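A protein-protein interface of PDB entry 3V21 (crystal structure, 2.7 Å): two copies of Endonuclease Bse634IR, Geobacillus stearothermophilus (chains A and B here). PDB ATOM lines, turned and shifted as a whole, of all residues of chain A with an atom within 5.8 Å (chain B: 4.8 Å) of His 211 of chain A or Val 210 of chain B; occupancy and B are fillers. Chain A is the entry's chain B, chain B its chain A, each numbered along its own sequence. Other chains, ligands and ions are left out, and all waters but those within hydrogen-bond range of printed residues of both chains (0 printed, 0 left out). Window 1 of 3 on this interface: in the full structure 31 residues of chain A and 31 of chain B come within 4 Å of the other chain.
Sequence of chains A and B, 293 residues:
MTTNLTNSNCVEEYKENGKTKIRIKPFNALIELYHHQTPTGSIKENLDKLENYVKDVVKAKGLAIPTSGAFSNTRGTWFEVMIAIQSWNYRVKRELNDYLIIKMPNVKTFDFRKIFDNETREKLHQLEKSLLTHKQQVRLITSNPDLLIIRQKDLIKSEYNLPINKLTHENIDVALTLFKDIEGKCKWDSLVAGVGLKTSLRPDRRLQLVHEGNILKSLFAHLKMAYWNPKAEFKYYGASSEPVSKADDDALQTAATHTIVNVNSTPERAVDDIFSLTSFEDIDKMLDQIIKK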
ATOM      1  N   ILE A 141      10.533  -3.869  15.241  1.00  0.00           N
ATOM      2  CA  ILE A 141      10.123  -5.000  16.050  1.00  0.00           C
ATOM      3  C   ILE A 141      10.727  -6.344  15.684  1.00  0.00           C
ATOM      4  O   ILE A 141      10.861  -6.701  14.509  1.00  0.00           O
ATOM      5  CB  ILE A 141       8.595  -5.139  16.040  1.00  0.00           C
ATOM      6  CG1 ILE A 141       7.977  -3.925  16.732  1.00  0.00           C
ATOM      7  CG2 ILE A 141       8.176  -6.441  16.706  1.00  0.00           C
ATOM      8  CD1 ILE A 141       6.473  -3.952  16.783  1.00  0.00           C
ATOM      9  N   THR A 142      11.088  -7.080  16.728  1.00  0.00           N
ATOM     10  CA  THR A 142      11.656  -8.404  16.606  1.00  0.00           C
ATOM     11  C   THR A 142      11.473  -9.093  17.953  1.00  0.00           C
ATOM     12  O   THR A 142      11.448  -8.448  19.016  1.00  0.00           O
ATOM     13  CB  THR A 142      13.175  -8.383  16.276  1.00  0.00           C
ATOM     14  OG1 THR A 142      13.639  -9.724  16.066  1.00  0.00           O
ATOM     15  CG2 THR A 142      13.971  -7.792  17.432  1.00  0.00           C
ATOM     16  N   SER A 143      11.331 -10.408  17.906  1.00  0.00           N
ATOM     17  CA  SER A 143      11.182 -11.186  19.116  1.00  0.00           C
ATOM     18  C   SER A 143      12.493 -11.094  19.903  1.00  0.00           C
ATOM     19  O   SER A 143      13.553 -10.907  19.313  1.00  0.00           O
ATOM     20  CB  SER A 143      10.881 -12.638  18.734  1.00  0.00           C
ATOM     21  OG  SER A 143      11.739 -13.083  17.694  1.00  0.00           O
ATOM     22  N   LEU A 207      15.201 -17.830   8.040  1.00  0.00           N
ATOM     23  CA  LEU A 207      15.231 -16.421   7.683  1.00  0.00           C
ATOM     24  C   LEU A 207      14.785 -15.557   8.853  1.00  0.00           C
ATOM     25  O   LEU A 207      14.924 -14.333   8.831  1.00  0.00           O
ATOM     26  CB  LEU A 207      14.329 -16.162   6.478  1.00  0.00           C
ATOM     27  CG  LEU A 207      14.722 -16.913   5.205  1.00  0.00           C
ATOM     28  CD1 LEU A 207      13.754 -16.578   4.078  1.00  0.00           C
ATOM     29  CD2 LEU A 207      16.140 -16.551   4.832  1.00  0.00           C
ATOM     30  N   GLN A 208      14.243 -16.197   9.882  1.00  0.00           N
ATOM     31  CA  GLN A 208      13.795 -15.460  11.053  1.00  0.00           C
ATOM     32  C   GLN A 208      15.035 -15.034  11.804  1.00  0.00           C
ATOM     33  O   GLN A 208      15.038 -14.008  12.476  1.00  0.00           O
ATOM     34  CB  GLN A 208      12.900 -16.331  11.929  1.00  0.00           C
ATOM     35  CG  GLN A 208      11.676 -16.846  11.168  1.00  0.00           C
ATOM     36  CD  GLN A 208      10.794 -17.752  11.999  1.00  0.00           C
ATOM     37  OE1 GLN A 208       9.943 -18.486  11.459  1.00  0.00           O
ATOM     38  NE2 GLN A 208      10.988 -17.702  13.331  1.00  0.00           N
ATOM     39  N   LEU A 209      16.090 -15.833  11.692  1.00  0.00           N
ATOM     40  CA  LEU A 209      17.359 -15.507  12.324  1.00  0.00           C
ATOM     41  C   LEU A 209      17.934 -14.256  11.651  1.00  0.00           C
ATOM     42  O   LEU A 209      18.392 -13.347  12.326  1.00  0.00           O
ATOM     43  CB  LEU A 209      18.338 -16.662  12.165  1.00  0.00           C
ATOM     44  CG  LEU A 209      18.030 -17.931  12.948  1.00  0.00           C
ATOM     45  CD1 LEU A 209      18.968 -19.046  12.517  1.00  0.00           C
ATOM     46  CD2 LEU A 209      18.167 -17.630  14.435  1.00  0.00           C
ATOM     47  N   VAL A 210      17.906 -14.207  10.323  1.00  0.00           N
ATOM     48  CA  VAL A 210      18.425 -13.053   9.596  1.00  0.00           C
ATOM     49  C   VAL A 210      17.663 -11.788   9.981  1.00  0.00           C
ATOM     50  O   VAL A 210      18.255 -10.713  10.146  1.00  0.00           O
ATOM     51  CB  VAL A 210      18.331 -13.257   8.049  1.00  0.00           C
ATOM     52  CG1 VAL A 210      18.834 -12.017   7.317  1.00  0.00           C
ATOM     53  CG2 VAL A 210      19.147 -14.463   7.640  1.00  0.00           C
ATOM     54  N   HIS A 211      16.348 -11.907  10.120  1.00  0.00           N
ATOM     55  CA  HIS A 211      15.540 -10.753  10.501  1.00  0.00           C
ATOM     56  C   HIS A 211      15.964 -10.294  11.893  1.00  0.00           C
ATOM     57  O   HIS A 211      16.171  -9.105  12.136  1.00  0.00           O
ATOM     58  CB  HIS A 211      14.056 -11.106  10.525  1.00  0.00           C
ATOM     59  CG  HIS A 211      13.211 -10.053  11.161  1.00  0.00           C
ATOM     60  ND1 HIS A 211      12.884  -8.877  10.522  1.00  0.00           N
ATOM     61  CD2 HIS A 211      12.683  -9.963  12.406  1.00  0.00           C
ATOM     62  CE1 HIS A 211      12.190  -8.109  11.348  1.00  0.00           C
ATOM     63  NE2 HIS A 211      12.056  -8.743  12.498  1.00  0.00           N
ATOM     64  N   GLU A 212      16.079 -11.249  12.808  1.00  0.00           N
ATOM     65  CA  GLU A 212      16.500 -10.962  14.168  1.00  0.00           C
ATOM     66  C   GLU A 212      17.809 -10.186  14.147  1.00  0.00           C
ATOM     67  O   GLU A 212      17.889  -9.039  14.587  1.00  0.00           O
ATOM     68  CB  GLU A 212      16.701 -12.268  14.923  1.00  0.00           C
ATOM     69  CG  GLU A 212      15.527 -12.659  15.764  1.00  0.00           C
ATOM     70  CD  GLU A 212      15.803 -12.424  17.230  1.00  0.00           C
ATOM     71  OE1 GLU A 212      16.181 -13.400  17.921  1.00  0.00           O
ATOM     72  OE2 GLU A 212      15.662 -11.266  17.689  1.00  0.00           O
ATOM     73  N   GLY A 213      18.842 -10.821  13.619  1.00  0.00           N
ATOM     74  CA  GLY A 213      20.133 -10.179  13.566  1.00  0.00           C
ATOM     75  C   GLY A 213      20.062  -8.823  12.917  1.00  0.00           C
ATOM     76  O   GLY A 213      20.689  -7.878  13.385  1.00  0.00           O
ATOM     77  N   ASN A 214      19.286  -8.717  11.845  1.00  0.00           N
ATOM     78  CA  ASN A 214      19.173  -7.451  11.141  1.00  0.00           C
ATOM     79  C   ASN A 214      18.581  -6.350  12.014  1.00  0.00           C
ATOM     80  O   ASN A 214      19.161  -5.271  12.123  1.00  0.00           O
ATOM     81  CB  ASN A 214      18.340  -7.621   9.866  1.00  0.00           C
ATOM     82  CG  ASN A 214      18.340  -6.368   8.998  1.00  0.00           C
ATOM     83  OD1 ASN A 214      19.378  -5.923   8.527  1.00  0.00           O
ATOM     84  ND2 ASN A 214      17.171  -5.796   8.791  1.00  0.00           N
ATOM     85  N   ILE A 215      17.433  -6.604  12.641  1.00  0.00           N
ATOM     86  CA  ILE A 215      16.811  -5.580  13.476  1.00  0.00           C
ATOM     87  C   ILE A 215      17.628  -5.275  14.724  1.00  0.00           C
ATOM     88  O   ILE A 215      17.699  -4.130  15.172  1.00  0.00           O
ATOM     89  CB  ILE A 215      15.381  -5.971  13.869  1.00  0.00           C
ATOM     90  CG1 ILE A 215      14.397  -5.527  12.785  1.00  0.00           C
ATOM     91  CG2 ILE A 215      14.992  -5.262  15.144  1.00  0.00           C
ATOM     92  CD1 ILE A 215      14.808  -5.879  11.404  1.00  0.00           C
ATOM     93  N   LEU A 216      18.250  -6.295  15.291  1.00  0.00           N
ATOM     94  CA  LEU A 216      19.085  -6.081  16.469  1.00  0.00           C
ATOM     95  C   LEU A 216      20.290  -5.218  16.096  1.00  0.00           C
ATOM     96  O   LEU A 216      20.581  -4.234  16.761  1.00  0.00           O
ATOM     97  CB  LEU A 216      19.569  -7.416  17.041  1.00  0.00           C
ATOM     98  CG  LEU A 216      18.525  -8.285  17.736  1.00  0.00           C
ATOM     99  CD1 LEU A 216      19.174  -9.578  18.168  1.00  0.00           C
ATOM    100  CD2 LEU A 216      17.953  -7.549  18.938  1.00  0.00           C
ATOM    101  N   ALA A 270      23.758 -10.391   8.807  1.00  0.00           N
ATOM    102  CA  ALA A 270      22.760 -10.231   9.844  1.00  0.00           C
ATOM    103  C   ALA A 270      23.152 -11.247  10.905  1.00  0.00           C
ATOM    104  O   ALA A 270      23.204 -10.933  12.093  1.00  0.00           O
ATOM    105  CB  ALA A 270      21.381 -10.530   9.295  1.00  0.00           C
ATOM    106  N   ARG B 206       5.225 -14.196  10.982  1.00  0.00           N
ATOM    107  CA  ARG B 206       4.938 -12.908  10.363  1.00  0.00           C
ATOM    108  C   ARG B 206       6.212 -12.110  10.098  1.00  0.00           C
ATOM    109  O   ARG B 206       6.255 -11.249   9.219  1.00  0.00           O
ATOM    110  CB  ARG B 206       3.971 -12.095  11.236  1.00  0.00           C
ATOM    111  CG  ARG B 206       4.557 -11.560  12.524  1.00  0.00           C
ATOM    112  CD  ARG B 206       3.472 -10.988  13.424  1.00  0.00           C
ATOM    113  NE  ARG B 206       4.018 -10.608  14.723  1.00  0.00           N
ATOM    114  CZ  ARG B 206       3.294 -10.444  15.828  1.00  0.00           C
ATOM    115  NH1 ARG B 206       1.983 -10.629  15.803  1.00  0.00           N
ATOM    116  NH2 ARG B 206       3.882 -10.093  16.958  1.00  0.00           N
ATOM    117  N   LEU B 207       7.267 -12.410  10.842  1.00  0.00           N
ATOM    118  CA  LEU B 207       8.513 -11.688  10.667  1.00  0.00           C
ATOM    119  C   LEU B 207       9.207 -12.100   9.386  1.00  0.00           C
ATOM    120  O   LEU B 207      10.116 -11.415   8.912  1.00  0.00           O
ATOM    121  CB  LEU B 207       9.422 -11.916  11.874  1.00  0.00           C
ATOM    122  CG  LEU B 207       8.853 -11.399  13.200  1.00  0.00           C
ATOM    123  CD1 LEU B 207       9.825 -11.709  14.309  1.00  0.00           C
ATOM    124  CD2 LEU B 207       8.579  -9.906  13.110  1.00  0.00           C
ATOM    125  N   GLN B 208       8.774 -13.219   8.818  1.00  0.00           N
ATOM    126  CA  GLN B 208       9.366 -13.698   7.579  1.00  0.00           C
ATOM    127  C   GLN B 208       8.941 -12.721   6.469  1.00  0.00           C
ATOM    128  O   GLN B 208       9.665 -12.490   5.504  1.00  0.00           O
ATOM    129  CB  GLN B 208       8.889 -15.121   7.301  1.00  0.00           C
ATOM    130  CG  GLN B 208       9.171 -16.069   8.453  1.00  0.00           C
ATOM    131  CD  GLN B 208       8.655 -17.475   8.197  1.00  0.00           C
ATOM    132  OE1 GLN B 208       8.472 -18.261   9.129  1.00  0.00           O
ATOM    133  NE2 GLN B 208       8.427 -17.799   6.933  1.00  0.00           N
ATOM    134  N   LEU B 209       7.769 -12.126   6.633  1.00  0.00           N
ATOM    135  CA  LEU B 209       7.276 -11.160   5.666  1.00  0.00           C
ATOM    136  C   LEU B 209       8.188  -9.933   5.677  1.00  0.00           C
ATOM    137  O   LEU B 209       8.543  -9.411   4.622  1.00  0.00           O
ATOM    138  CB  LEU B 209       5.834 -10.741   6.016  1.00  0.00           C
ATOM    139  CG  LEU B 209       4.713 -11.767   5.835  1.00  0.00           C
ATOM    140  CD1 LEU B 209       3.428 -11.250   6.415  1.00  0.00           C
ATOM    141  CD2 LEU B 209       4.545 -12.055   4.362  1.00  0.00           C
ATOM    142  N   VAL B 210       8.562  -9.483   6.880  1.00  0.00           N
ATOM    143  CA  VAL B 210       9.430  -8.315   7.039  1.00  0.00           C
ATOM    144  C   VAL B 210      10.779  -8.593   6.406  1.00  0.00           C
ATOM    145  O   VAL B 210      11.354  -7.747   5.732  1.00  0.00           O
ATOM    146  CB  VAL B 210       9.646  -7.960   8.521  1.00  0.00           C
ATOM    147  CG1 VAL B 210      10.583  -6.786   8.621  1.00  0.00           C
ATOM    148  CG2 VAL B 210       8.311  -7.605   9.185  1.00  0.00           C
ATOM    149  N   HIS B 211      11.283  -9.795   6.618  1.00  0.00           N
ATOM    150  CA  HIS B 211      12.555 -10.149   6.032  1.00  0.00           C
ATOM    151  C   HIS B 211      12.423 -10.109   4.523  1.00  0.00           C
ATOM    152  O   HIS B 211      13.256  -9.527   3.832  1.00  0.00           O
ATOM    153  CB  HIS B 211      12.979 -11.550   6.446  1.00  0.00           C
ATOM    154  CG  HIS B 211      14.142 -12.061   5.667  1.00  0.00           C
ATOM    155  ND1 HIS B 211      15.433 -11.655   5.911  1.00  0.00           N
ATOM    156  CD2 HIS B 211      14.201 -12.884   4.595  1.00  0.00           C
ATOM    157  CE1 HIS B 211      16.241 -12.207   5.024  1.00  0.00           C
ATOM    158  NE2 HIS B 211      15.518 -12.956   4.213  1.00  0.00           N
ATOM    159  N   GLU B 212      11.366 -10.735   4.020  1.00  0.00           N
ATOM    160  CA  GLU B 212      11.116 -10.805   2.584  1.00  0.00           C
ATOM    161  C   GLU B 212      11.031  -9.420   1.938  1.00  0.00           C
ATOM    162  O   GLU B 212      11.639  -9.171   0.898  1.00  0.00           O
ATOM    163  CB  GLU B 212       9.827 -11.599   2.328  1.00  0.00           C
ATOM    164  CG  GLU B 212       9.509 -11.894   0.855  1.00  0.00           C
ATOM    165  CD  GLU B 212      10.285 -13.079   0.282  1.00  0.00           C
ATOM    166  OE1 GLU B 212      10.049 -14.228   0.732  1.00  0.00           O
ATOM    167  OE2 GLU B 212      11.127 -12.856  -0.621  1.00  0.00           O
ATOM    168  N   GLY B 213      10.271  -8.520   2.547  1.00  0.00           N
ATOM    169  CA  GLY B 213      10.148  -7.180   2.004  1.00  0.00           C
ATOM    170  C   GLY B 213      11.456  -6.425   2.127  1.00  0.00           C
ATOM    171  O   GLY B 213      11.823  -5.647   1.255  1.00  0.00           O
ATOM    172  N   ASN B 214      12.172  -6.662   3.220  1.00  0.00           N
ATOM    173  CA  ASN B 214      13.439  -5.996   3.445  1.00  0.00           C
ATOM    174  C   ASN B 214      14.485  -6.385   2.394  1.00  0.00           C
ATOM    175  O   ASN B 214      15.072  -5.522   1.765  1.00  0.00           O
ATOM    176  CB  ASN B 214      13.951  -6.321   4.848  1.00  0.00           C
ATOM    177  CG  ASN B 214      15.189  -5.528   5.210  1.00  0.00           C
ATOM    178  OD1 ASN B 214      15.159  -4.294   5.258  1.00  0.00           O
ATOM    179  ND2 ASN B 214      16.292  -6.230   5.458  1.00  0.00           N
ATOM    180  N   ALA B 251       4.092  -5.286  14.257  1.00  0.00           N
ATOM    181  CA  ALA B 251       5.234  -6.059  13.791  1.00  0.00           C
ATOM    182  C   ALA B 251       5.497  -5.790  12.322  1.00  0.00           C
ATOM    183  O   ALA B 251       6.641  -5.596  11.917  1.00  0.00           O
ATOM    184  CB  ALA B 251       4.981  -7.528  13.998  1.00  0.00           C
ATOM    185  N   LEU B 252       4.426  -5.766  11.529  1.00  0.00           N
ATOM    186  CA  LEU B 252       4.530  -5.531  10.092  1.00  0.00           C
ATOM    187  C   LEU B 252       4.752  -4.064   9.684  1.00  0.00           C
ATOM    188  O   LEU B 252       4.694  -3.716   8.497  1.00  0.00           O
ATOM    189  CB  LEU B 252       3.308  -6.114   9.390  1.00  0.00           C
ATOM    190  CG  LEU B 252       3.223  -7.637   9.558  1.00  0.00           C
ATOM    191  CD1 LEU B 252       1.922  -8.158   8.979  1.00  0.00           C
ATOM    192  CD2 LEU B 252       4.416  -8.285   8.882  1.00  0.00           C
ATOM    193  N   THR B 254       7.510  -2.742  10.795  1.00  0.00           N
ATOM    194  CA  THR B 254       8.958  -2.723  10.953  1.00  0.00           C
ATOM    195  C   THR B 254       9.624  -2.041   9.766  1.00  0.00           C
ATOM    196  O   THR B 254       9.335  -2.357   8.614  1.00  0.00           O
ATOM    197  CB  THR B 254       9.524  -4.143  11.116  1.00  0.00           C
ATOM    198  OG1 THR B 254       8.757  -4.854  12.094  1.00  0.00           O
ATOM    199  CG2 THR B 254      10.975  -4.088  11.563  1.00  0.00           C
ATOM    200  N   ALA B 270       9.184  -2.420   5.694  1.00  0.00           N
ATOM    201  CA  ALA B 270       9.589  -3.593   4.935  1.00  0.00           C
ATOM    202  C   ALA B 270       8.309  -4.050   4.230  1.00  0.00           C
ATOM    203  O   ALA B 270       8.297  -4.316   3.025  1.00  0.00           O
ATOM    204  CB  ALA B 270      10.111  -4.680   5.871  1.00  0.00           C
ATOM    205  N   VAL B 271       7.226  -4.124   5.002  1.00  0.00           N
ATOM    206  CA  VAL B 271       5.919  -4.518   4.480  1.00  0.00           C
ATOM    207  C   VAL B 271       5.044  -3.263   4.506  1.00  0.00           C
ATOM    208  O   VAL B 271       4.675  -2.752   5.576  1.00  0.00           O
ATOM    209  CB  VAL B 271       5.279  -5.618   5.353  1.00  0.00           C
ATOM    210  CG1 VAL B 271       3.946  -6.016   4.779  1.00  0.00           C
ATOM    211  CG2 VAL B 271       6.203  -6.825   5.439  1.00  0.00           C
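The side-chain amide oxygen (OE1) of Gln 208 of chain A sits close to the side-chain amide oxygen (OE1) of Gln 208 of chain B, 2.8 Å away.
The side-chain amide nitrogen (ND2) of Asn 214 of chain B sits close to the side-chain amide nitrogen (ND2) of Asn 214 of chain A (3.5 Å).
The backbone carbonyl oxygen (O) of Ile 141 of chain A sits at hydrogen-bond distance from a ring nitrogen (NE2) of His 211 of chain A, at 3.1 Å.
O of Thr 254 of chain B lies within hydrogen-bond range of N of Ala 270 of chain B, at 2.9 Å.
Among the printed residues, pairs that only touch across the chains: Ile 141 of chain A with Ala 251 of chain B (3.7 Å), Ile 141 of chain A with Thr 254 of chain B (3.7 Å), Leu 207 of chain A with His 211 of chain B (3.7 Å), Val 210 of chain A with His 211 of chain B (3.5 Å), His 211 of chain A with Leu 207 of chain B (3.7 Å), His 211 of chain A with Val 210 of chain B (3.4 Å) and Ile 215 of chain A with Thr 254 of chain B (3.9 Å).
Printed residues of chain A within 4 Å of Val 210 of chain B: His 211 (3.4 Å).
Printed residues of chain A within 4 Å of Gln 208 of chain B: Gln 208.
Of the printed residues of chain A, Leu 207 of chain B touches His 211 (3.7 Å).
Printed residues of chain B within 4 Å of Ile 215 of chain A: Thr 254.
Printed residues of chain B within 4 Å of Val 210 of chain A: His 211 (3.5 Å).
Gly 213 of chain A touches none of the printed residues of chain B.
The nearest residue of chain B that does not touch His 211 of chain A is Thr 254 of chain B (4.2 Å).
The nearest printed residue of chain B that does not touch Leu 207 of chain A is Glu 212 of chain B (5.5 Å).
Of the 14 printed residues of chain A, 7 touch a printed residue of chain B.
Along chain A the printed residues that touch a printed residue of chain B span positions 141 to 215.
Along chain B the printed residues that touch a printed residue of chain A span positions 207 to 254.
Among the printed residues, no Asp or Glu carboxylate lies within 4 Å of a Lys or Arg side-chain nitrogen of the other chain.
Leu 207 of chain A touches His 211 of chain B, and with the chains exchanged His 211 of chain A touches Leu 207 of chain B.
Gln 208 of chain B touches its own counterpart, Gln 208 of chain A.
Val 210 of chain A touches His 211 of chain B, and with the chains exchanged His 211 of chain A touches Val 210 of chain B.
Asn 214 of chain A touches its own counterpart, Asn 214 of chain B.
9 positions are printed for both chains.
Of the 9 pairs that touch across the chains among the printed residues, 6 have their exchanged pair printed and touching as well.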
